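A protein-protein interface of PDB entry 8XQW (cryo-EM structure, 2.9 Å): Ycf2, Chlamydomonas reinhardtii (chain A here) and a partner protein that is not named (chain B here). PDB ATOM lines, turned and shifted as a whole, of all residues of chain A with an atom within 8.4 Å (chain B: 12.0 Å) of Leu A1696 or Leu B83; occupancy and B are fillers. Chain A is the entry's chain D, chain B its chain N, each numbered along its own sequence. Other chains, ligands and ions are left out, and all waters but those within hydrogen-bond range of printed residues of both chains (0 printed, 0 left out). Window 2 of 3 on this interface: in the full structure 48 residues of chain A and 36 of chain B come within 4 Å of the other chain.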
ATOM      1  N   LYS A1689     -36.670 -11.335  23.665  1.00  0.00           N
ATOM      2  CA  LYS A1689     -36.592 -10.126  22.856  1.00  0.00           C
ATOM      3  C   LYS A1689     -35.817  -9.028  23.553  1.00  0.00           C
ATOM      4  O   LYS A1689     -35.169  -8.217  22.891  1.00  0.00           O
ATOM      5  CB  LYS A1689     -37.984  -9.624  22.515  1.00  0.00           C
ATOM      6  CG  LYS A1689     -38.552 -10.197  21.256  1.00  0.00           C
ATOM      7  CD  LYS A1689     -39.990  -9.814  21.123  1.00  0.00           C
ATOM      8  CE  LYS A1689     -40.657 -10.636  20.060  1.00  0.00           C
ATOM      9  NZ  LYS A1689     -42.114 -10.365  19.993  1.00  0.00           N
ATOM     10  N   TYR A1691     -33.185  -9.350  25.680  1.00  0.00           N
ATOM     11  CA  TYR A1691     -31.752  -9.564  25.843  1.00  0.00           C
ATOM     12  C   TYR A1691     -31.062 -10.111  24.605  1.00  0.00           C
ATOM     13  O   TYR A1691     -29.982 -10.686  24.726  1.00  0.00           O
ATOM     14  CB  TYR A1691     -31.492 -10.494  27.021  1.00  0.00           C
ATOM     15  CG  TYR A1691     -31.657  -9.795  28.332  1.00  0.00           C
ATOM     16  CD1 TYR A1691     -30.828  -8.756  28.690  1.00  0.00           C
ATOM     17  CD2 TYR A1691     -32.664 -10.152  29.198  1.00  0.00           C
ATOM     18  CE1 TYR A1691     -30.990  -8.108  29.876  1.00  0.00           C
ATOM     19  CE2 TYR A1691     -32.835  -9.507  30.384  1.00  0.00           C
ATOM     20  CZ  TYR A1691     -31.996  -8.487  30.721  1.00  0.00           C
ATOM     21  OH  TYR A1691     -32.168  -7.844  31.917  1.00  0.00           O
ATOM     22  N   ARG A1692     -31.631  -9.931  23.422  1.00  0.00           N
ATOM     23  CA  ARG A1692     -31.060 -10.553  22.239  1.00  0.00           C
ATOM     24  C   ARG A1692     -30.028  -9.692  21.545  1.00  0.00           C
ATOM     25  O   ARG A1692     -29.367 -10.176  20.624  1.00  0.00           O
ATOM     26  CB  ARG A1692     -32.150 -10.907  21.239  1.00  0.00           C
ATOM     27  CG  ARG A1692     -32.519  -9.777  20.343  1.00  0.00           C
ATOM     28  CD  ARG A1692     -33.663 -10.175  19.472  1.00  0.00           C
ATOM     29  NE  ARG A1692     -34.581  -9.069  19.270  1.00  0.00           N
ATOM     30  CZ  ARG A1692     -35.725  -9.178  18.617  1.00  0.00           C
ATOM     31  NH1 ARG A1692     -36.071 -10.342  18.099  1.00  0.00           N
ATOM     32  NH2 ARG A1692     -36.511  -8.131  18.480  1.00  0.00           N
ATOM     33  N   THR A1693     -29.867  -8.440  21.946  1.00  0.00           N
ATOM     34  CA  THR A1693     -28.909  -7.555  21.308  1.00  0.00           C
ATOM     35  C   THR A1693     -27.613  -7.441  22.090  1.00  0.00           C
ATOM     36  O   THR A1693     -26.806  -6.555  21.808  1.00  0.00           O
ATOM     37  CB  THR A1693     -29.520  -6.176  21.117  1.00  0.00           C
ATOM     38  OG1 THR A1693     -28.611  -5.360  20.377  1.00  0.00           O
ATOM     39  CG2 THR A1693     -29.767  -5.537  22.454  1.00  0.00           C
ATOM     40  N   ILE A1694     -27.390  -8.323  23.054  1.00  0.00           N
ATOM     41  CA  ILE A1694     -26.240  -8.242  23.945  1.00  0.00           C
ATOM     42  C   ILE A1694     -24.933  -8.580  23.237  1.00  0.00           C
ATOM     43  O   ILE A1694     -23.934  -7.895  23.481  1.00  0.00           O
ATOM     44  CB  ILE A1694     -26.444  -9.142  25.170  1.00  0.00           C
ATOM     45  CG1 ILE A1694     -27.157  -8.366  26.262  1.00  0.00           C
ATOM     46  CG2 ILE A1694     -25.125  -9.676  25.674  1.00  0.00           C
ATOM     47  CD1 ILE A1694     -27.278  -9.122  27.515  1.00  0.00           C
ATOM     48  N   PRO A1695     -24.859  -9.609  22.387  1.00  0.00           N
ATOM     49  CA  PRO A1695     -23.571  -9.883  21.731  1.00  0.00           C
ATOM     50  C   PRO A1695     -23.056  -8.733  20.885  1.00  0.00           C
ATOM     51  O   PRO A1695     -21.886  -8.358  21.005  1.00  0.00           O
ATOM     52  CB  PRO A1695     -23.875 -11.129  20.894  1.00  0.00           C
ATOM     53  CG  PRO A1695     -25.329 -11.191  20.809  1.00  0.00           C
ATOM     54  CD  PRO A1695     -25.821 -10.677  22.092  1.00  0.00           C
ATOM     55  N   LEU A1696     -23.899  -8.151  20.040  1.00  0.00           N
ATOM     56  CA  LEU A1696     -23.444  -7.057  19.192  1.00  0.00           C
ATOM     57  C   LEU A1696     -23.097  -5.825  20.014  1.00  0.00           C
ATOM     58  O   LEU A1696     -22.105  -5.147  19.739  1.00  0.00           O
ATOM     59  CB  LEU A1696     -24.515  -6.732  18.159  1.00  0.00           C
ATOM     60  CG  LEU A1696     -24.023  -6.234  16.807  1.00  0.00           C
ATOM     61  CD1 LEU A1696     -22.850  -7.047  16.362  1.00  0.00           C
ATOM     62  CD2 LEU A1696     -25.129  -6.321  15.794  1.00  0.00           C
ATOM     63  N   SER A1697     -23.898  -5.526  21.032  1.00  0.00           N
ATOM     64  CA  SER A1697     -23.610  -4.397  21.908  1.00  0.00           C
ATOM     65  C   SER A1697     -22.274  -4.565  22.615  1.00  0.00           C
ATOM     66  O   SER A1697     -21.438  -3.658  22.596  1.00  0.00           O
ATOM     67  CB  SER A1697     -24.738  -4.249  22.923  1.00  0.00           C
ATOM     68  OG  SER A1697     -24.396  -3.335  23.937  1.00  0.00           O
ATOM     69  N   PHE A1698     -22.067  -5.716  23.249  1.00  0.00           N
ATOM     70  CA  PHE A1698     -20.806  -6.021  23.918  1.00  0.00           C
ATOM     71  C   PHE A1698     -19.627  -5.906  22.959  1.00  0.00           C
ATOM     72  O   PHE A1698     -18.615  -5.263  23.269  1.00  0.00           O
ATOM     73  CB  PHE A1698     -20.911  -7.425  24.510  1.00  0.00           C
ATOM     74  CG  PHE A1698     -19.696  -7.891  25.244  1.00  0.00           C
ATOM     75  CD1 PHE A1698     -18.597  -8.369  24.570  1.00  0.00           C
ATOM     76  CD2 PHE A1698     -19.677  -7.909  26.615  1.00  0.00           C
ATOM     77  CE1 PHE A1698     -17.498  -8.815  25.247  1.00  0.00           C
ATOM     78  CE2 PHE A1698     -18.577  -8.357  27.292  1.00  0.00           C
ATOM     79  CZ  PHE A1698     -17.489  -8.809  26.606  1.00  0.00           C
ATOM     80  N   ILE A1699     -19.738  -6.524  21.783  1.00  0.00           N
ATOM     81  CA  ILE A1699     -18.645  -6.508  20.818  1.00  0.00           C
ATOM     82  C   ILE A1699     -18.311  -5.081  20.411  1.00  0.00           C
ATOM     83  O   ILE A1699     -17.142  -4.685  20.380  1.00  0.00           O
ATOM     84  CB  ILE A1699     -19.006  -7.366  19.593  1.00  0.00           C
ATOM     85  CG1 ILE A1699     -18.673  -8.826  19.853  1.00  0.00           C
ATOM     86  CG2 ILE A1699     -18.283  -6.876  18.358  1.00  0.00           C
ATOM     87  CD1 ILE A1699     -17.241  -9.152  19.605  1.00  0.00           C
ATOM     88  N   SER A1700     -19.330  -4.288  20.086  1.00  0.00           N
ATOM     89  CA  SER A1700     -19.068  -2.940  19.603  1.00  0.00           C
ATOM     90  C   SER A1700     -18.567  -2.034  20.713  1.00  0.00           C
ATOM     91  O   SER A1700     -17.881  -1.046  20.439  1.00  0.00           O
ATOM     92  CB  SER A1700     -20.326  -2.356  18.983  1.00  0.00           C
ATOM     93  OG  SER A1700     -21.114  -1.746  19.984  1.00  0.00           O
ATOM     94  N   THR A1701     -18.905  -2.338  21.961  1.00  0.00           N
ATOM     95  CA  THR A1701     -18.358  -1.567  23.067  1.00  0.00           C
ATOM     96  C   THR A1701     -16.879  -1.856  23.253  1.00  0.00           C
ATOM     97  O   THR A1701     -16.048  -0.944  23.219  1.00  0.00           O
ATOM     98  CB  THR A1701     -19.120  -1.879  24.346  1.00  0.00           C
ATOM     99  OG1 THR A1701     -20.383  -1.211  24.317  1.00  0.00           O
ATOM    100  CG2 THR A1701     -18.332  -1.418  25.545  1.00  0.00           C
ATOM    101  N   THR A1702     -16.524  -3.127  23.429  1.00  0.00           N
ATOM    102  CA  THR A1702     -15.160  -3.449  23.822  1.00  0.00           C
ATOM    103  C   THR A1702     -14.143  -3.216  22.712  1.00  0.00           C
ATOM    104  O   THR A1702     -12.943  -3.160  22.995  1.00  0.00           O
ATOM    105  CB  THR A1702     -15.092  -4.894  24.308  1.00  0.00           C
ATOM    106  OG1 THR A1702     -16.236  -5.164  25.120  1.00  0.00           O
ATOM    107  CG2 THR A1702     -13.872  -5.103  25.162  1.00  0.00           C
ATOM    108  N   LEU A1703     -14.577  -3.066  21.468  1.00  0.00           N
ATOM    109  CA  LEU A1703     -13.653  -2.833  20.356  1.00  0.00           C
ATOM    110  C   LEU A1703     -13.501  -1.341  20.071  1.00  0.00           C
ATOM    111  O   LEU A1703     -13.782  -0.858  18.974  1.00  0.00           O
ATOM    112  CB  LEU A1703     -14.125  -3.576  19.113  1.00  0.00           C
ATOM    113  CG  LEU A1703     -13.201  -4.684  18.630  1.00  0.00           C
ATOM    114  CD1 LEU A1703     -13.672  -5.202  17.294  1.00  0.00           C
ATOM    115  CD2 LEU A1703     -11.788  -4.167  18.536  1.00  0.00           C
ATOM    116  N   LEU A1737     -15.215 -12.484  20.831  1.00  0.00           N
ATOM    117  CA  LEU A1737     -16.312 -13.295  20.317  1.00  0.00           C
ATOM    118  C   LEU A1737     -16.733 -14.361  21.321  1.00  0.00           C
ATOM    119  O   LEU A1737     -17.935 -14.565  21.567  1.00  0.00           O
ATOM    120  CB  LEU A1737     -15.905 -13.938  18.999  1.00  0.00           C
ATOM    121  CG  LEU A1737     -16.030 -13.077  17.753  1.00  0.00           C
ATOM    122  CD1 LEU A1737     -15.814 -13.932  16.545  1.00  0.00           C
ATOM    123  CD2 LEU A1737     -17.378 -12.432  17.695  1.00  0.00           C
ATOM    124  N   SER A1740     -18.676 -12.791  24.225  1.00  0.00           N
ATOM    125  CA  SER A1740     -20.030 -12.408  23.845  1.00  0.00           C
ATOM    126  C   SER A1740     -20.960 -13.608  23.855  1.00  0.00           C
ATOM    127  O   SER A1740     -22.044 -13.568  24.450  1.00  0.00           O
ATOM    128  CB  SER A1740     -20.016 -11.772  22.467  1.00  0.00           C
ATOM    129  OG  SER A1740     -19.261 -10.587  22.484  1.00  0.00           O
ATOM    130  N   HIS A1741     -20.546 -14.689  23.199  1.00  0.00           N
ATOM    131  CA  HIS A1741     -21.394 -15.874  23.140  1.00  0.00           C
ATOM    132  C   HIS A1741     -21.668 -16.428  24.529  1.00  0.00           C
ATOM    133  O   HIS A1741     -22.821 -16.695  24.894  1.00  0.00           O
ATOM    134  CB  HIS A1741     -20.741 -16.934  22.264  1.00  0.00           C
ATOM    135  CG  HIS A1741     -21.652 -18.058  21.902  1.00  0.00           C
ATOM    136  ND1 HIS A1741     -22.653 -17.930  20.967  1.00  0.00           N
ATOM    137  CD2 HIS A1741     -21.721 -19.329  22.355  1.00  0.00           C
ATOM    138  CE1 HIS A1741     -23.299 -19.073  20.859  1.00  0.00           C
ATOM    139  NE2 HIS A1741     -22.754 -19.939  21.691  1.00  0.00           N
ATOM    140  N   HIS A1744     -24.102 -14.146  26.631  1.00  0.00           N
ATOM    141  CA  HIS A1744     -25.498 -14.254  26.224  1.00  0.00           C
ATOM    142  C   HIS A1744     -26.112 -15.562  26.706  1.00  0.00           C
ATOM    143  O   HIS A1744     -27.215 -15.577  27.282  1.00  0.00           O
ATOM    144  CB  HIS A1744     -25.599 -14.134  24.711  1.00  0.00           C
ATOM    145  CG  HIS A1744     -26.998 -14.059  24.201  1.00  0.00           C
ATOM    146  ND1 HIS A1744     -27.384 -14.618  23.005  1.00  0.00           N
ATOM    147  CD2 HIS A1744     -28.107 -13.488  24.721  1.00  0.00           C
ATOM    148  CE1 HIS A1744     -28.671 -14.402  22.816  1.00  0.00           C
ATOM    149  NE2 HIS A1744     -29.133 -13.715  23.841  1.00  0.00           N
ATOM    150  N   ALA B  74     -25.979   8.836  26.985  1.00  0.00           N
ATOM    151  CA  ALA B  74     -27.323   8.427  26.592  1.00  0.00           C
ATOM    152  C   ALA B  74     -27.392   7.951  25.150  1.00  0.00           C
ATOM    153  O   ALA B  74     -28.218   7.090  24.823  1.00  0.00           O
ATOM    154  CB  ALA B  74     -28.308   9.577  26.792  1.00  0.00           C
ATOM    155  N   GLY B  75     -26.543   8.495  24.280  1.00  0.00           N
ATOM    156  CA  GLY B  75     -26.509   8.032  22.908  1.00  0.00           C
ATOM    157  C   GLY B  75     -26.106   6.581  22.794  1.00  0.00           C
ATOM    158  O   GLY B  75     -26.572   5.875  21.901  1.00  0.00           O
ATOM    159  N   TRP B  76     -25.242   6.116  23.692  1.00  0.00           N
ATOM    160  CA  TRP B  76     -24.914   4.692  23.703  1.00  0.00           C
ATOM    161  C   TRP B  76     -26.169   3.833  23.860  1.00  0.00           C
ATOM    162  O   TRP B  76     -26.429   2.923  23.058  1.00  0.00           O
ATOM    163  CB  TRP B  76     -23.921   4.403  24.818  1.00  0.00           C
ATOM    164  CG  TRP B  76     -23.343   3.055  24.751  1.00  0.00           C
ATOM    165  CD1 TRP B  76     -22.247   2.674  24.047  1.00  0.00           C
ATOM    166  CD2 TRP B  76     -23.816   1.887  25.419  1.00  0.00           C
ATOM    167  NE1 TRP B  76     -22.009   1.338  24.227  1.00  0.00           N
ATOM    168  CE2 TRP B  76     -22.961   0.831  25.068  1.00  0.00           C
ATOM    169  CE3 TRP B  76     -24.883   1.628  26.277  1.00  0.00           C
ATOM    170  CZ2 TRP B  76     -23.138  -0.459  25.549  1.00  0.00           C
ATOM    171  CZ3 TRP B  76     -25.059   0.346  26.748  1.00  0.00           C
ATOM    172  CH2 TRP B  76     -24.193  -0.680  26.386  1.00  0.00           C
ATOM    173  N   HIS B  77     -26.963   4.111  24.893  1.00  0.00           N
ATOM    174  CA  HIS B  77     -28.176   3.337  25.129  1.00  0.00           C
ATOM    175  C   HIS B  77     -29.155   3.478  23.977  1.00  0.00           C
ATOM    176  O   HIS B  77     -29.842   2.516  23.616  1.00  0.00           O
ATOM    177  CB  HIS B  77     -28.839   3.784  26.427  1.00  0.00           C
ATOM    178  CG  HIS B  77     -28.237   3.190  27.657  1.00  0.00           C
ATOM    179  ND1 HIS B  77     -27.347   3.873  28.454  1.00  0.00           N
ATOM    180  CD2 HIS B  77     -28.421   1.986  28.245  1.00  0.00           C
ATOM    181  CE1 HIS B  77     -26.999   3.110  29.473  1.00  0.00           C
ATOM    182  NE2 HIS B  77     -27.633   1.959  29.367  1.00  0.00           N
ATOM    183  N   LEU B  78     -29.254   4.674  23.399  1.00  0.00           N
ATOM    184  CA  LEU B  78     -30.190   4.858  22.294  1.00  0.00           C
ATOM    185  C   LEU B  78     -29.785   4.034  21.084  1.00  0.00           C
ATOM    186  O   LEU B  78     -30.640   3.479  20.389  1.00  0.00           O
ATOM    187  CB  LEU B  78     -30.295   6.330  21.922  1.00  0.00           C
ATOM    188  CG  LEU B  78     -31.122   7.161  22.890  1.00  0.00           C
ATOM    189  CD1 LEU B  78     -31.055   8.622  22.503  1.00  0.00           C
ATOM    190  CD2 LEU B  78     -32.557   6.670  22.925  1.00  0.00           C
ATOM    191  N   ALA B  79     -28.484   3.954  20.807  1.00  0.00           N
ATOM    192  CA  ALA B  79     -28.021   3.108  19.717  1.00  0.00           C
ATOM    193  C   ALA B  79     -28.377   1.655  19.975  1.00  0.00           C
ATOM    194  O   ALA B  79     -28.841   0.949  19.068  1.00  0.00           O
ATOM    195  CB  ALA B  79     -26.519   3.265  19.531  1.00  0.00           C
ATOM    196  N   SER B  80     -28.176   1.187  21.204  1.00  0.00           N
ATOM    197  CA  SER B  80     -28.549  -0.191  21.509  1.00  0.00           C
ATOM    198  C   SER B  80     -30.039  -0.425  21.293  1.00  0.00           C
ATOM    199  O   SER B  80     -30.446  -1.463  20.752  1.00  0.00           O
ATOM    200  CB  SER B  80     -28.161  -0.540  22.939  1.00  0.00           C
ATOM    201  OG  SER B  80     -29.102  -1.434  23.497  1.00  0.00           O
ATOM    202  N   PHE B  81     -30.872   0.534  21.698  1.00  0.00           N
ATOM    203  CA  PHE B  81     -32.316   0.367  21.556  1.00  0.00           C
ATOM    204  C   PHE B  81     -32.740   0.388  20.096  1.00  0.00           C
ATOM    205  O   PHE B  81     -33.644  -0.351  19.698  1.00  0.00           O
ATOM    206  CB  PHE B  81     -33.047   1.454  22.327  1.00  0.00           C
ATOM    207  CG  PHE B  81     -34.533   1.345  22.255  1.00  0.00           C
ATOM    208  CD1 PHE B  81     -35.172   0.201  22.677  1.00  0.00           C
ATOM    209  CD2 PHE B  81     -35.293   2.386  21.772  1.00  0.00           C
ATOM    210  CE1 PHE B  81     -36.530   0.097  22.612  1.00  0.00           C
ATOM    211  CE2 PHE B  81     -36.654   2.283  21.706  1.00  0.00           C
ATOM    212  CZ  PHE B  81     -37.273   1.140  22.128  1.00  0.00           C
ATOM    213  N   ALA B  82     -32.108   1.227  19.279  1.00  0.00           N
ATOM    214  CA  ALA B  82     -32.427   1.240  17.857  1.00  0.00           C
ATOM    215  C   ALA B  82     -32.042  -0.072  17.199  1.00  0.00           C
ATOM    216  O   ALA B  82     -32.777  -0.592  16.349  1.00  0.00           O
ATOM    217  CB  ALA B  82     -31.724   2.402  17.171  1.00  0.00           C
ATOM    218  N   LEU B  83     -30.886  -0.618  17.566  1.00  0.00           N
ATOM    219  CA  LEU B  83     -30.512  -1.929  17.053  1.00  0.00           C
ATOM    220  C   LEU B  83     -31.543  -2.980  17.423  1.00  0.00           C
ATOM    221  O   LEU B  83     -31.966  -3.765  16.575  1.00  0.00           O
ATOM    222  CB  LEU B  83     -29.147  -2.323  17.584  1.00  0.00           C
ATOM    223  CG  LEU B  83     -28.378  -3.274  16.686  1.00  0.00           C
ATOM    224  CD1 LEU B  83     -27.852  -2.520  15.494  1.00  0.00           C
ATOM    225  CD2 LEU B  83     -27.252  -3.890  17.466  1.00  0.00           C
ATOM    226  N   ASN B  84     -31.961  -3.013  18.685  1.00  0.00           N
ATOM    227  CA  ASN B  84     -32.975  -3.984  19.088  1.00  0.00           C
ATOM    228  C   ASN B  84     -34.289  -3.749  18.360  1.00  0.00           C
ATOM    229  O   ASN B  84     -35.074  -4.680  18.169  1.00  0.00           O
ATOM    230  CB  ASN B  84     -33.190  -3.926  20.593  1.00  0.00           C
ATOM    231  CG  ASN B  84     -33.727  -5.212  21.144  1.00  0.00           C
ATOM    232  OD1 ASN B  84     -34.153  -6.081  20.400  1.00  0.00           O
ATOM    233  ND2 ASN B  84     -33.718  -5.341  22.455  1.00  0.00           N
ATOM    234  N   LEU B  85     -34.560  -2.507  17.973  1.00  0.00           N
ATOM    235  CA  LEU B  85     -35.755  -2.223  17.189  1.00  0.00           C
ATOM    236  C   LEU B  85     -35.662  -2.812  15.795  1.00  0.00           C
ATOM    237  O   LEU B  85     -36.656  -3.314  15.266  1.00  0.00           O
ATOM    238  CB  LEU B  85     -35.966  -0.719  17.083  1.00  0.00           C
ATOM    239  CG  LEU B  85     -36.978  -0.068  18.000  1.00  0.00           C
ATOM    240  CD1 LEU B  85     -37.205   1.345  17.548  1.00  0.00           C
ATOM    241  CD2 LEU B  85     -38.248  -0.849  17.941  1.00  0.00           C
ATOM    242  N   ALA B  86     -34.484  -2.737  15.177  1.00  0.00           N
ATOM    243  CA  ALA B  86     -34.344  -3.195  13.798  1.00  0.00           C
ATOM    244  C   ALA B  86     -34.706  -4.663  13.636  1.00  0.00           C
ATOM    245  O   ALA B  86     -35.101  -5.079  12.548  1.00  0.00           O
ATOM    246  CB  ALA B  86     -32.925  -2.956  13.296  1.00  0.00           C
ATOM    247  N   PHE B  87     -34.567  -5.464  14.687  1.00  0.00           N
ATOM    248  CA  PHE B  87     -34.908  -6.877  14.591  1.00  0.00           C
ATOM    249  C   PHE B  87     -36.379  -7.059  14.271  1.00  0.00           C
ATOM    250  O   PHE B  87     -36.740  -7.602  13.226  1.00  0.00           O
ATOM    251  CB  PHE B  87     -34.578  -7.579  15.895  1.00  0.00           C
ATOM    252  CG  PHE B  87     -33.209  -8.154  15.957  1.00  0.00           C
ATOM    253  CD1 PHE B  87     -32.940  -9.383  15.407  1.00  0.00           C
ATOM    254  CD2 PHE B  87     -32.203  -7.491  16.610  1.00  0.00           C
ATOM    255  CE1 PHE B  87     -31.695  -9.913  15.483  1.00  0.00           C
ATOM    256  CE2 PHE B  87     -30.958  -8.023  16.691  1.00  0.00           C
ATOM    257  CZ  PHE B  87     -30.706  -9.235  16.130  1.00  0.00           C
ATOM    258  N   TRP B  88     -37.238  -6.629  15.183  1.00  0.00           N
ATOM    259  CA  TRP B  88     -38.690  -6.556  15.109  1.00  0.00           C
ATOM    260  C   TRP B  88     -39.383  -7.901  15.304  1.00  0.00           C
ATOM    261  O   TRP B  88     -40.598  -7.923  15.444  1.00  0.00           O
ATOM    262  CB  TRP B  88     -39.197  -5.934  13.796  1.00  0.00           C
ATOM    263  CG  TRP B  88     -40.585  -5.463  13.903  1.00  0.00           C
ATOM    264  CD1 TRP B  88     -41.690  -6.062  13.400  1.00  0.00           C
ATOM    265  CD2 TRP B  88     -41.033  -4.300  14.593  1.00  0.00           C
ATOM    266  NE1 TRP B  88     -42.806  -5.339  13.723  1.00  0.00           N
ATOM    267  CE2 TRP B  88     -42.428  -4.249  14.459  1.00  0.00           C
ATOM    268  CE3 TRP B  88     -40.390  -3.294  15.309  1.00  0.00           C
ATOM    269  CZ2 TRP B  88     -43.185  -3.233  15.008  1.00  0.00           C
ATOM    270  CZ3 TRP B  88     -41.144  -2.292  15.856  1.00  0.00           C
ATOM    271  CH2 TRP B  88     -42.526  -2.264  15.704  1.00  0.00           C
ATOM    272  N   GLY B  89     -38.674  -9.015  15.359  1.00  0.00           N
ATOM    273  CA  GLY B  89     -39.392 -10.264  15.498  1.00  0.00           C
ATOM    274  C   GLY B  89     -38.578 -11.512  15.250  1.00  0.00           C
ATOM    275  O   GLY B  89     -37.498 -11.686  15.820  1.00  0.00           O
ATOM    276  N   VAL B  90     -39.091 -12.402  14.408  1.00  0.00           N
ATOM    277  CA  VAL B  90     -38.455 -13.693  14.196  1.00  0.00           C
ATOM    278  C   VAL B  90     -38.218 -13.934  12.713  1.00  0.00           C
ATOM    279  O   VAL B  90     -37.541 -14.896  12.335  1.00  0.00           O
ATOM    280  CB  VAL B  90     -39.302 -14.826  14.795  1.00  0.00           C
ATOM    281  CG1 VAL B  90     -39.593 -14.550  16.255  1.00  0.00           C
ATOM    282  CG2 VAL B  90     -40.587 -14.986  14.011  1.00  0.00           C
ATOM    283  N   GLU B  91     -38.801 -13.141  11.861  1.00  0.00           N
ATOM    284  CA  GLU B  91     -38.653 -13.336  10.450  1.00  0.00           C
ATOM    285  C   GLU B  91     -37.245 -13.216  10.064  1.00  0.00           C
ATOM    286  O   GLU B  91     -36.805 -12.200   9.897  1.00  0.00           O
ATOM    287  CB  GLU B  91     -39.441 -12.266   9.798  1.00  0.00           C
ATOM    288  CG  GLU B  91     -39.048 -11.859   8.426  1.00  0.00           C
ATOM    289  CD  GLU B  91     -40.205 -11.161   7.757  1.00  0.00           C
ATOM    290  OE1 GLU B  91     -41.281 -11.755   7.732  1.00  0.00           O
ATOM    291  OE2 GLU B  91     -40.082 -10.031   7.272  1.00  0.00           O
ATOM    292  N   MET B  93     -35.127 -15.586  11.538  1.00  0.00           N
ATOM    293  CA  MET B  93     -34.613 -16.572  12.464  1.00  0.00           C
ATOM    294  C   MET B  93     -35.249 -17.927  12.204  1.00  0.00           C
ATOM    295  O   MET B  93     -36.477 -18.054  12.241  1.00  0.00           O
ATOM    296  CB  MET B  93     -34.881 -16.170  13.917  1.00  0.00           C
ATOM    297  CG  MET B  93     -34.604 -14.720  14.217  1.00  0.00           C
ATOM    298  SD  MET B  93     -32.882 -14.418  14.616  1.00  0.00           S
ATOM    299  CE  MET B  93     -32.482 -13.179  13.394  1.00  0.00           C
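O of Lys A1689 is in hydrogen-bond range of ND2 of Asn B84 (3.3 Å). NE1 of Trp B76 sits at hydrogen-bond distance from OG1 of Thr A1701 (3.0 Å). The side-chain amide oxygen (OD1) of Asn B84 is in hydrogen-bond range of the guanidinium group (NE) of Arg A1692 (3.2 Å). NH1 of Arg A1692 sits at hydrogen-bond distance from O of Gly B89.
The backbone carbonyl oxygen (O) of Ser A1697 lies within hydrogen-bond range of the side-chain hydroxyl (OG) of Ser A1700, 3.3 Å away. O of Ser A1697 sits at hydrogen-bond distance from OG1 of Thr A1701, 3.2 Å away.
Among the printed residues, merely in contact across the chains: Arg A1692 with Phe B87, Arg A1692 with Trp B88, Thr A1693 with Leu B83, Thr A1693 with Asn B84, Leu A1696 with Leu B83 and Ser A1697 with Trp B76.
Printed residues of chain B within 4 Å of Lys A1689: Asn B84. Thr A1693 touches just these residues of chain B: Leu B83 (3.5 Å) and Asn B84 (3.96 Å). No residue of chain B comes within 4 Å of Pro A1695. Leu A1696 touches one residue of chain B. Ser A1697 touches one residue of chain B. No residue of chain B comes within 4 Å of Ile A1699. Printed residues of chain B within 4 Å of Thr A1701: Trp B76 (3.0 Å). Ala B82 touches none of the printed residues of chain A. Leu B83 touches just these residues of chain A: Thr A1693 and Leu A1696. Printed residues of chain A within 4 Å of Phe B87: Arg A1692. Of the printed residues of chain A, Trp B88 touches Arg A1692. The nearest residue of chain B that does not touch Leu A1696 is Phe B87 (6.1 Å). The nearest printed residue of chain B that does not touch Arg A1692 is Val B90 (5.2 Å).
Hydrophobic or aromatic side chains of chain A within 4 Å of the printed part of chain B: Leu A1696. Printed residues of chain B that touch a printed residue of chain A: Trp B76, Leu B83, Asn B84, Phe B87, Trp B88 and Gly B89. Hydrophobic or aromatic side chains of chain B within 4 Å of the printed part of chain A: Trp B76, Leu B83 and Phe B87. Along chain B the printed residues that touch a printed residue of chain A span positions 76 to 89. Among the printed residues, 10 pairs touch across the chains. Among the printed residues, no Asp or Glu carboxylate lies within 4 Å of a Lys or Arg side-chain nitrogen of the other chain.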
